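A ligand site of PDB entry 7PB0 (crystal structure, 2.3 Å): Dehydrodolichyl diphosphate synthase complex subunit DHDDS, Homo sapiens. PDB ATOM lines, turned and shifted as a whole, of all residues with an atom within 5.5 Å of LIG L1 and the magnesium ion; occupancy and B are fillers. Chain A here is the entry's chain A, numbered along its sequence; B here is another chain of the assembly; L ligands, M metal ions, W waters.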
ATOM      1  N   ILE A  39       3.371  11.517 -19.820  1.00  0.00           N
ATOM      2  CA  ILE A  39       2.330  10.807 -19.089  1.00  0.00           C
ATOM      3  C   ILE A  39       2.399  11.288 -17.648  1.00  0.00           C
ATOM      4  O   ILE A  39       3.304  10.909 -16.895  1.00  0.00           O
ATOM      5  CB  ILE A  39       2.481   9.288 -19.177  1.00  0.00           C
ATOM      6  CG1 ILE A  39       2.531   8.859 -20.652  1.00  0.00           C
ATOM      7  CG2 ILE A  39       1.327   8.602 -18.444  1.00  0.00           C
ATOM      8  CD1 ILE A  39       2.887   7.404 -20.848  1.00  0.00           C
ATOM      9  N   MET A  40       1.443  12.120 -17.245  1.00  0.00           N
ATOM     10  CA  MET A  40       1.509  12.808 -15.964  1.00  0.00           C
ATOM     11  C   MET A  40       0.870  11.931 -14.881  1.00  0.00           C
ATOM     12  O   MET A  40      -0.270  12.111 -14.475  1.00  0.00           O
ATOM     13  CB  MET A  40       0.824  14.157 -16.063  1.00  0.00           C
ATOM     14  CG  MET A  40       1.396  15.022 -17.170  1.00  0.00           C
ATOM     15  SD  MET A  40       0.410  16.517 -17.353  1.00  0.00           S
ATOM     16  CE  MET A  40      -1.052  15.841 -18.137  1.00  0.00           C
ATOM     17  N   ASP A  41       1.661  10.992 -14.377  1.00  0.00           N
ATOM     18  CA  ASP A  41       1.161   9.942 -13.497  1.00  0.00           C
ATOM     19  C   ASP A  41       1.643  10.140 -12.069  1.00  0.00           C
ATOM     20  O   ASP A  41       2.753  10.628 -11.820  1.00  0.00           O
ATOM     21  CB  ASP A  41       1.603   8.571 -14.014  1.00  0.00           C
ATOM     22  CG  ASP A  41       0.887   7.439 -13.316  1.00  0.00           C
ATOM     23  OD1 ASP A  41      -0.095   7.717 -12.602  1.00  0.00           O
ATOM     24  OD2 ASP A  41       1.327   6.271 -13.485  1.00  0.00           O
ATOM     25  N   GLY A  42       0.792   9.760 -11.115  1.00  0.00           N
ATOM     26  CA  GLY A  42       1.132   9.743  -9.713  1.00  0.00           C
ATOM     27  C   GLY A  42       0.453  10.795  -8.854  1.00  0.00           C
ATOM     28  O   GLY A  42       0.885  11.010  -7.708  1.00  0.00           O
ATOM     29  N   ARG A  44      -2.470  10.812  -7.378  1.00  0.00           N
ATOM     30  CA  ARG A  44      -3.208  10.342  -6.203  1.00  0.00           C
ATOM     31  C   ARG A  44      -2.268   9.853  -5.109  1.00  0.00           C
ATOM     32  O   ARG A  44      -2.522  10.108  -3.928  1.00  0.00           O
ATOM     33  CB  ARG A  44      -4.193   9.242  -6.617  1.00  0.00           C
ATOM     34  CG  ARG A  44      -5.254   9.707  -7.626  1.00  0.00           C
ATOM     35  CD  ARG A  44      -6.341   8.630  -7.854  1.00  0.00           C
ATOM     36  NE  ARG A  44      -5.803   7.455  -8.539  1.00  0.00           N
ATOM     37  CZ  ARG A  44      -6.513   6.387  -8.877  1.00  0.00           C
ATOM     38  NH1 ARG A  44      -7.812   6.320  -8.601  1.00  0.00           N
ATOM     39  NH2 ARG A  44      -5.932   5.366  -9.495  1.00  0.00           N
ATOM     40  N   ARG A  45      -1.184   9.172  -5.478  1.00  0.00           N
ATOM     41  CA  ARG A  45      -0.194   8.781  -4.473  1.00  0.00           C
ATOM     42  C   ARG A  45       0.397  10.014  -3.795  1.00  0.00           C
ATOM     43  O   ARG A  45       0.631  10.024  -2.579  1.00  0.00           O
ATOM     44  CB  ARG A  45       0.903   7.932  -5.112  1.00  0.00           C
ATOM     45  CG  ARG A  45       0.499   6.491  -5.363  1.00  0.00           C
ATOM     46  CD  ARG A  45       1.413   5.850  -6.396  1.00  0.00           C
ATOM     47  NE  ARG A  45       0.982   6.125  -7.767  1.00  0.00           N
ATOM     48  CZ  ARG A  45       1.701   5.817  -8.848  1.00  0.00           C
ATOM     49  NH1 ARG A  45       2.871   5.214  -8.722  1.00  0.00           N
ATOM     50  NH2 ARG A  45       1.238   6.112 -10.061  1.00  0.00           N
ATOM     51  N   TYR A  83      -0.849  13.463 -21.657  1.00  0.00           N
ATOM     52  CA  TYR A  83      -1.940  12.538 -21.388  1.00  0.00           C
ATOM     53  C   TYR A  83      -2.746  13.111 -20.221  1.00  0.00           C
ATOM     54  O   TYR A  83      -2.314  13.043 -19.063  1.00  0.00           O
ATOM     55  CB  TYR A  83      -1.406  11.151 -21.077  1.00  0.00           C
ATOM     56  CG  TYR A  83      -2.307   9.998 -21.461  1.00  0.00           C
ATOM     57  CD1 TYR A  83      -1.874   8.686 -21.325  1.00  0.00           C
ATOM     58  CD2 TYR A  83      -3.588  10.219 -21.975  1.00  0.00           C
ATOM     59  CE1 TYR A  83      -2.688   7.615 -21.689  1.00  0.00           C
ATOM     60  CE2 TYR A  83      -4.408   9.155 -22.341  1.00  0.00           C
ATOM     61  CZ  TYR A  83      -3.952   7.856 -22.186  1.00  0.00           C
ATOM     62  OH  TYR A  83      -4.759   6.792 -22.548  1.00  0.00           O
ATOM     63  N   ALA A  84      -3.896  13.693 -20.510  1.00  0.00           N
ATOM     64  CA  ALA A  84      -4.698  14.301 -19.459  1.00  0.00           C
ATOM     65  C   ALA A  84      -5.856  13.420 -18.992  1.00  0.00           C
ATOM     66  O   ALA A  84      -6.279  13.533 -17.837  1.00  0.00           O
ATOM     67  CB  ALA A  84      -5.246  15.662 -19.902  1.00  0.00           C
ATOM     68  N   PHE A  85      -6.384  12.555 -19.850  1.00  0.00           N
ATOM     69  CA  PHE A  85      -7.479  11.686 -19.435  1.00  0.00           C
ATOM     70  C   PHE A  85      -7.591  10.516 -20.379  1.00  0.00           C
ATOM     71  O   PHE A  85      -7.805  10.703 -21.589  1.00  0.00           O
ATOM     72  CB  PHE A  85      -8.794  12.463 -19.380  1.00  0.00           C
ATOM     73  CG  PHE A  85      -9.872  11.767 -18.588  1.00  0.00           C
ATOM     74  CD1 PHE A  85     -10.814  10.965 -19.221  1.00  0.00           C
ATOM     75  CD2 PHE A  85      -9.929  11.900 -17.210  1.00  0.00           C
ATOM     76  CE1 PHE A  85     -11.796  10.316 -18.503  1.00  0.00           C
ATOM     77  CE2 PHE A  85     -10.917  11.265 -16.473  1.00  0.00           C
ATOM     78  CZ  PHE A  85     -11.853  10.463 -17.125  1.00  0.00           C
ATOM     79  N   SER A  86      -7.474   9.312 -19.845  1.00  0.00           N
ATOM     80  CA  SER A  86      -7.627   8.113 -20.634  1.00  0.00           C
ATOM     81  C   SER A  86      -9.084   7.686 -20.676  1.00  0.00           C
ATOM     82  O   SER A  86      -9.831   7.876 -19.720  1.00  0.00           O
ATOM     83  CB  SER A  86      -6.762   6.987 -20.061  1.00  0.00           C
ATOM     84  OG  SER A  86      -7.066   5.758 -20.702  1.00  0.00           O
ATOM     85  N   ASN A  89      -9.816   5.844 -17.830  1.00  0.00           N
ATOM     86  CA  ASN A  89     -10.073   6.551 -16.588  1.00  0.00           C
ATOM     87  C   ASN A  89     -11.563   6.759 -16.337  1.00  0.00           C
ATOM     88  O   ASN A  89     -11.955   7.055 -15.205  1.00  0.00           O
ATOM     89  CB  ASN A  89      -9.353   7.897 -16.565  1.00  0.00           C
ATOM     90  CG  ASN A  89      -7.848   7.743 -16.557  1.00  0.00           C
ATOM     91  OD1 ASN A  89      -7.115   8.576 -17.078  1.00  0.00           O
ATOM     92  ND2 ASN A  89      -7.383   6.645 -15.954  1.00  0.00           N
ATOM     93  N   ARG A  92     -13.188   5.032 -13.242  1.00  0.00           N
ATOM     94  CA  ARG A  92     -13.035   5.433 -11.856  1.00  0.00           C
ATOM     95  C   ARG A  92     -14.378   5.867 -11.290  1.00  0.00           C
ATOM     96  O   ARG A  92     -15.381   5.959 -11.991  1.00  0.00           O
ATOM     97  CB  ARG A  92     -12.003   6.562 -11.744  1.00  0.00           C
ATOM     98  CG  ARG A  92     -10.641   6.169 -12.271  1.00  0.00           C
ATOM     99  CD  ARG A  92      -9.632   7.299 -12.178  1.00  0.00           C
ATOM    100  NE  ARG A  92      -8.286   6.820 -12.457  1.00  0.00           N
ATOM    101  CZ  ARG A  92      -7.179   7.528 -12.242  1.00  0.00           C
ATOM    102  NH1 ARG A  92      -7.269   8.759 -11.760  1.00  0.00           N
ATOM    103  NH2 ARG A  92      -5.995   7.006 -12.513  1.00  0.00           N
ATOM    104  N   ARG A 212       7.278   9.256 -18.599  1.00  0.00           N
ATOM    105  CA  ARG A 212       6.257   8.819 -17.662  1.00  0.00           C
ATOM    106  C   ARG A 212       6.799   8.915 -16.244  1.00  0.00           C
ATOM    107  O   ARG A 212       7.885   8.399 -15.956  1.00  0.00           O
ATOM    108  CB  ARG A 212       5.791   7.395 -17.946  1.00  0.00           C
ATOM    109  CG  ARG A 212       4.835   6.891 -16.879  1.00  0.00           C
ATOM    110  CD  ARG A 212       3.927   5.817 -17.383  1.00  0.00           C
ATOM    111  NE  ARG A 212       2.756   5.648 -16.520  1.00  0.00           N
ATOM    112  CZ  ARG A 212       1.750   4.817 -16.805  1.00  0.00           C
ATOM    113  NH1 ARG A 212       1.790   4.074 -17.900  1.00  0.00           N
ATOM    114  NH2 ARG A 212       0.716   4.728 -15.980  1.00  0.00           N
ATOM    115  N   GLU A 216       6.071   3.671 -12.722  1.00  0.00           N
ATOM    116  CA  GLU A 216       5.525   2.707 -13.671  1.00  0.00           C
ATOM    117  C   GLU A 216       6.366   2.637 -14.945  1.00  0.00           C
ATOM    118  O   GLU A 216       6.713   3.676 -15.517  1.00  0.00           O
ATOM    119  CB  GLU A 216       4.079   3.053 -14.020  1.00  0.00           C
ATOM    120  CG  GLU A 216       3.174   3.289 -12.823  1.00  0.00           C
ATOM    121  CD  GLU A 216       3.291   2.187 -11.781  1.00  0.00           C
ATOM    122  OE1 GLU A 216       3.399   1.004 -12.161  1.00  0.00           O
ATOM    123  OE2 GLU A 216       3.269   2.504 -10.572  1.00  0.00           O
ATOM    124  N   ARG A 218       5.449   1.365 -18.035  1.00  0.00           N
ATOM    125  CA  ARG A 218       4.544   0.961 -19.113  1.00  0.00           C
ATOM    126  C   ARG A 218       4.004   2.217 -19.785  1.00  0.00           C
ATOM    127  O   ARG A 218       4.147   3.333 -19.275  1.00  0.00           O
ATOM    128  CB  ARG A 218       3.399   0.086 -18.577  1.00  0.00           C
ATOM    129  CG  ARG A 218       2.781   0.587 -17.292  1.00  0.00           C
ATOM    130  CD  ARG A 218       1.458  -0.132 -16.978  1.00  0.00           C
ATOM    131  NE  ARG A 218       0.787   0.471 -15.828  1.00  0.00           N
ATOM    132  CZ  ARG A 218       1.049   0.154 -14.558  1.00  0.00           C
ATOM    133  NH1 ARG A 218       1.974  -0.766 -14.283  1.00  0.00           N
ATOM    134  NH2 ARG A 218       0.390   0.744 -13.574  1.00  0.00           N
ATOM    135  N   SER A 220       0.677   2.540 -21.058  1.00  0.00           N
ATOM    136  CA  SER A 220      -0.750   2.725 -20.796  1.00  0.00           C
ATOM    137  C   SER A 220      -1.489   3.335 -21.979  1.00  0.00           C
ATOM    138  O   SER A 220      -2.247   4.296 -21.847  1.00  0.00           O
ATOM    139  CB  SER A 220      -0.960   3.551 -19.527  1.00  0.00           C
ATOM    140  OG  SER A 220      -0.836   2.737 -18.367  1.00  0.00           O
ATOM    141  N   LEU B 186       0.007  -2.143 -22.562  1.00  0.00           N
ATOM    142  CA  LEU B 186       0.121  -2.314 -21.112  1.00  0.00           C
ATOM    143  C   LEU B 186       1.354  -3.120 -20.719  1.00  0.00           C
ATOM    144  O   LEU B 186       1.512  -3.460 -19.539  1.00  0.00           O
ATOM    145  CB  LEU B 186      -1.141  -2.959 -20.555  1.00  0.00           C
ATOM    146  CG  LEU B 186      -2.382  -2.057 -20.528  1.00  0.00           C
ATOM    147  CD1 LEU B 186      -3.606  -2.823 -20.031  1.00  0.00           C
ATOM    148  CD2 LEU B 186      -2.134  -0.821 -19.663  1.00  0.00           C
ATOM    149  N   GLU B 214       2.281  -3.378 -10.211  1.00  0.00           N
ATOM    150  CA  GLU B 214       0.866  -3.230  -9.923  1.00  0.00           C
ATOM    151  C   GLU B 214       0.204  -2.538 -11.101  1.00  0.00           C
ATOM    152  O   GLU B 214       0.587  -1.431 -11.470  1.00  0.00           O
ATOM    153  CB  GLU B 214       0.652  -2.454  -8.624  1.00  0.00           C
ATOM    154  N   GLN B 215      -0.770  -3.212 -11.714  1.00  0.00           N
ATOM    155  CA  GLN B 215      -1.462  -2.696 -12.891  1.00  0.00           C
ATOM    156  C   GLN B 215      -2.889  -2.364 -12.503  1.00  0.00           C
ATOM    157  O   GLN B 215      -3.668  -3.251 -12.157  1.00  0.00           O
ATOM    158  CB  GLN B 215      -1.446  -3.721 -14.036  1.00  0.00           C
ATOM    159  CG  GLN B 215      -0.038  -4.129 -14.526  1.00  0.00           C
ATOM    160  CD  GLN B 215       0.142  -5.657 -14.593  1.00  0.00           C
ATOM    161  OE1 GLN B 215      -0.563  -6.401 -13.904  1.00  0.00           O
ATOM    162  NE2 GLN B 215       1.050  -6.115 -15.460  1.00  0.00           N
ATOM    163  N   ARG B 216      -3.236  -1.084 -12.588  1.00  0.00           N
ATOM    164  CA  ARG B 216      -4.531  -0.601 -12.133  1.00  0.00           C
ATOM    165  C   ARG B 216      -5.546  -0.435 -13.263  1.00  0.00           C
ATOM    166  O   ARG B 216      -6.726  -0.245 -12.977  1.00  0.00           O
ATOM    167  CB  ARG B 216      -4.354   0.717 -11.378  1.00  0.00           C
ATOM    168  CG  ARG B 216      -3.532   0.563 -10.104  1.00  0.00           C
ATOM    169  CD  ARG B 216      -3.150   1.910  -9.479  1.00  0.00           C
ATOM    170  NE  ARG B 216      -1.969   2.508 -10.086  1.00  0.00           N
ATOM    171  CZ  ARG B 216      -0.711   2.156  -9.802  1.00  0.00           C
ATOM    172  NH1 ARG B 216      -0.473   1.192  -8.919  1.00  0.00           N
ATOM    173  NH2 ARG B 216       0.304   2.760 -10.403  1.00  0.00           N
ATOM    174  N   LEU B 217      -5.095  -0.498 -14.514  1.00  0.00           N
ATOM    175  CA  LEU B 217      -5.977  -0.513 -15.680  1.00  0.00           C
ATOM    176  C   LEU B 217      -6.862   0.723 -15.753  1.00  0.00           C
ATOM    177  O   LEU B 217      -8.003   0.662 -16.205  1.00  0.00           O
ATOM    178  CB  LEU B 217      -6.841  -1.783 -15.712  1.00  0.00           C
ATOM    179  CG  LEU B 217      -6.108  -3.113 -15.512  1.00  0.00           C
ATOM    180  CD1 LEU B 217      -7.109  -4.232 -15.285  1.00  0.00           C
ATOM    181  CD2 LEU B 217      -5.210  -3.434 -16.701  1.00  0.00           C
ATOM    182  N   GLY B 218      -6.338   1.875 -15.321  1.00  0.00           N
ATOM    183  CA  GLY B 218      -7.077   3.120 -15.384  1.00  0.00           C
ATOM    184  C   GLY B 218      -7.878   3.458 -14.151  1.00  0.00           C
ATOM    185  O   GLY B 218      -8.228   4.630 -13.962  1.00  0.00           O
ATOM    186  N   LYS B 219      -8.161   2.478 -13.303  1.00  0.00           N
ATOM    187  CA  LYS B 219      -8.933   2.716 -12.080  1.00  0.00           C
ATOM    188  C   LYS B 219      -8.076   3.320 -10.967  1.00  0.00           C
ATOM    189  O   LYS B 219      -8.604   3.777  -9.946  1.00  0.00           O
ATOM    190  CB  LYS B 219      -9.586   1.413 -11.582  1.00  0.00           C
ATOM    191  CG  LYS B 219     -10.831   1.004 -12.334  1.00  0.00           C
ATOM    192  CD  LYS B 219     -11.320  -0.361 -11.883  1.00  0.00           C
ATOM    193  OXT LYS B 219      -6.842   3.346 -11.065  1.00  0.00           O
HETATM  194  P1  LIG L   1      -2.480   2.667 -15.245  1.00  0.00           P
HETATM  195  O1  LIG L   1      -2.195   4.127 -15.958  1.00  0.00           O
HETATM  196  P2  LIG L   1      -2.753   5.594 -15.419  1.00  0.00           P
HETATM  197  O2  LIG L   1      -2.362   1.595 -16.300  1.00  0.00           O
HETATM  198  O3  LIG L   1      -3.879   2.664 -14.654  1.00  0.00           O
HETATM  199  O4  LIG L   1      -1.495   2.417 -14.125  1.00  0.00           O
HETATM  200  O5  LIG L   1      -2.520   5.743 -13.929  1.00  0.00           O
HETATM  201  O6  LIG L   1      -4.213   5.735 -15.772  1.00  0.00           O
HETATM  202  S1  LIG L   1      -1.652   7.132 -16.376  1.00  0.00           S
HETATM  203  C1  LIG L   1      -2.319   7.466 -18.031  1.00  0.00           C
HETATM  204  C2  LIG L   1      -3.653   8.201 -17.929  1.00  0.00           C
HETATM  205  C3  LIG L   1      -3.434   9.714 -17.849  1.00  0.00           C
HETATM  206  C4  LIG L   1      -2.043  10.304 -17.577  1.00  0.00           C
HETATM  207  C5  LIG L   1      -4.462  10.524 -18.012  1.00  0.00           C
HETATM  208  C1  LG2 L   2      -3.048  10.439 -13.798  1.00  0.00           C
HETATM  209  S1  LG2 L   2      -2.345  10.633 -12.164  1.00  0.00           S
HETATM  210  C2  LG2 L   2      -3.140  11.785 -14.472  1.00  0.00           C
HETATM  211  C3  LG2 L   2      -4.259  12.254 -14.909  1.00  0.00           C
HETATM  212  C4  LG2 L   2      -5.535  11.443 -14.758  1.00  0.00           C
HETATM  213  C5  LG2 L   2      -4.234  13.610 -15.574  1.00  0.00           C
HETATM  214  C6  LG2 L   2      -4.461  14.721 -14.568  1.00  0.00           C
HETATM  215  C7  LG2 L   2      -3.392  15.773 -14.760  1.00  0.00           C
HETATM  216  C8  LG2 L   2      -3.714  17.025 -15.006  1.00  0.00           C
HETATM  217  C9  LG2 L   2      -5.177  17.426 -15.129  1.00  0.00           C
HETATM  218  P1  LG2 L   2      -3.357   9.134 -11.113  1.00  0.00           P
HETATM  219  P2  LG2 L   2      -1.942   7.560  -9.274  1.00  0.00           P
HETATM  220  C10 LG2 L   2      -2.609  18.047 -15.176  1.00  0.00           C
HETATM  221  C11 LG2 L   2      -5.292  18.809 -15.801  1.00  0.00           C
HETATM  222  C12 LG2 L   2      -4.550  18.785 -17.130  1.00  0.00           C
HETATM  223  C13 LG2 L   2      -4.950  19.515 -18.132  1.00  0.00           C
HETATM  224  C14 LG2 L   2      -4.204  19.484 -19.450  1.00  0.00           C
HETATM  225  C15 LG2 L   2      -6.178  20.394 -17.994  1.00  0.00           C
HETATM  226  C16 LG2 L   2      -7.377  19.557 -18.410  1.00  0.00           C
HETATM  227  C17 LG2 L   2      -7.732  18.620 -17.269  1.00  0.00           C
HETATM  228  C18 LG2 L   2      -8.485  17.574 -17.506  1.00  0.00           C
HETATM  229  C19 LG2 L   2      -9.016  17.286 -18.909  1.00  0.00           C
HETATM  230  O1  LG2 L   2      -3.316   7.879 -11.887  1.00  0.00           O
HETATM  231  O2  LG2 L   2      -1.372   6.919 -10.481  1.00  0.00           O
HETATM  232  C20 LG2 L   2      -8.835  16.643 -16.353  1.00  0.00           C
HETATM  233  O3  LG2 L   2      -4.769   9.545 -10.953  1.00  0.00           O
HETATM  234  O4  LG2 L   2      -2.939   6.686  -8.623  1.00  0.00           O
HETATM  235  O5  LG2 L   2      -2.680   8.928  -9.688  1.00  0.00           O
HETATM  236  O6  LG2 L   2      -0.917   7.868  -8.271  1.00  0.00           O
HETATM  237 MG    MG M   1      -1.640   6.505 -12.374  1.00  0.00          MG
HETATM  238  O   HOH W   1      -4.130   1.662 -18.308  1.00  0.00           O
HETATM  239  O   HOH W   2      -0.340   4.768 -12.578  1.00  0.00           O
HETATM  240  O   HOH W   3      -3.268   4.936 -11.347  1.00  0.00           O
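OD2 of Asp 41 lies within salt-bridge range of NH2 of Arg 212 (3.0 Å). The guanidinium group (NH1) of Arg 212 lies within hydrogen-bond range of the backbone carbonyl oxygen (O) of Arg 218 of chain A, at 2.8 Å. NH2 of Arg 218 of chain A is in hydrogen-bond range of O of Glu 214 of chain B, 3.0 Å away. The side-chain amide nitrogen of Asn 89 lies within hydrogen-bond range of the backbone carbonyl oxygen of Gly 218 of chain B (3.0 Å). NE of Arg 92 is in hydrogen-bond range of O of Gly 218 of chain B (2.7 Å). The side-chain hydroxyl (OH) of Tyr 83 sits at hydrogen-bond distance from the side-chain hydroxyl (OG) of Ser 86, at 3.1 Å. OE2 of Glu 216 of chain A is in salt-bridge range of NH1 of Arg 45. O of Lys 219 of chain B lies within salt-bridge range of NE of Arg 92, at 3.96 Å.
The guanidinium group of Arg 218 of chain A is in salt-bridge range of an oxygen (O4) of LIG L1, 2.6 Å away. An oxygen (O3) of LIG L1 is in hydrogen-bond range of the backbone NH of Gly 218 of chain B, at 2.7 Å. The side-chain hydroxyl (OG) of Ser 220 is in hydrogen-bond range of an oxygen (O2) of LIG L1 (2.8 Å). NH2 of Arg 212 is in salt-bridge range of O4 of LIG L1 (3.7 Å). The side-chain amide nitrogen (ND2) of Asn 89 sits at hydrogen-bond distance from an oxygen (O6) of LIG L1 (3.3 Å). N of Leu 217 of chain B lies within hydrogen-bond range of O3 of LIG L1, at 3.4 Å. O6 of LIG L1 is in salt-bridge range of NH2 of Arg 92 (3.9 Å). The backbone NH (N) of Arg 45 sits at hydrogen-bond distance from an oxygen (O6) of LG2 L2, 3.1 Å away. An oxygen (O6) of LG2 L2 lies within salt-bridge range of the guanidinium group of Arg 45 (2.6 Å). NH1 of Arg 92 lies within salt-bridge range of O3 of LG2 L2. The backbone NH of Gly 42 lies close to a sulfur (S1) of LG2 L2 (3.4 Å). N of Arg 44 sits at hydrogen-bond distance from O5 of LG2 L2, 3.0 Å away. The guanidinium group (NE) of Arg 44 lies within salt-bridge range of an oxygen (O4) of LG2 L2, 3.0 Å away.
Water W2 lies within hydrogen-bond range of the side-chain carboxylate of Asp 41, the guanidinium group of Arg 216 of chain B, an oxygen (O4) of LIG L1 and the guanidinium group of Arg 45. Water W3 lies within hydrogen-bond range of NE of Arg 216 of chain B (3.0 Å), O4 of LG2 L2 (3.3 Å) and NH2 of Arg 44 (3.3 Å). Water W1 lies within hydrogen-bond range of O2 of LIG L1 (2.7 Å) and OG of Ser 220 (3.5 Å).
Arg 45 touches the magnesium ion (NH2 to MG, 3.7 Å). The nearest printed residue that does not touch the magnesium ion is Gly 42 (4.3 Å).
The magnesium ion is bound by an oxygen (O5) of LIG L1 (1.9 Å), an oxygen (O2) of LG2 L2 (2.0 Å), the side-chain carboxylate (OD1) of Asp 41 (2.0 Å), water W2 (2.2 Å), an oxygen (O1) of LG2 L2 (2.2 Å) and water W3 (2.5 Å). The magnesium ion has six donor atoms within binding distance.
CG2 of Ile 39 touches C1 of LIG L1 (3.8 Å). N of Met 40 touches C4 of LIG L1, at 3.9 Å. O of Tyr 83 touches C4 of LIG L1 (3.1 Å). Ala 84 touches LIG L1 (C to C5, 3.4 Å). Phe 85 touches LIG L1. Ser 86 touches LIG L1 (N to C5, 3.7 Å). Arg 216 of chain B touches LIG L1. Hydrophobic or aromatic side chains within 4 Å of LIG L1: Ile 39 and Tyr 83. Within 4 Å of LIG L1: Ile 39, Met 40, Asp 41, Tyr 83, Ala 84, Phe 85, Ser 86, Asn 89, Arg 92, Arg 212, Arg 218 of chain A, Ser 220, Arg 216 of chain B, Leu 217 of chain B and Gly 218 of chain B. The nearest printed residue that does not touch LIG L1 is Leu 186 of chain B (4.1 Å).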
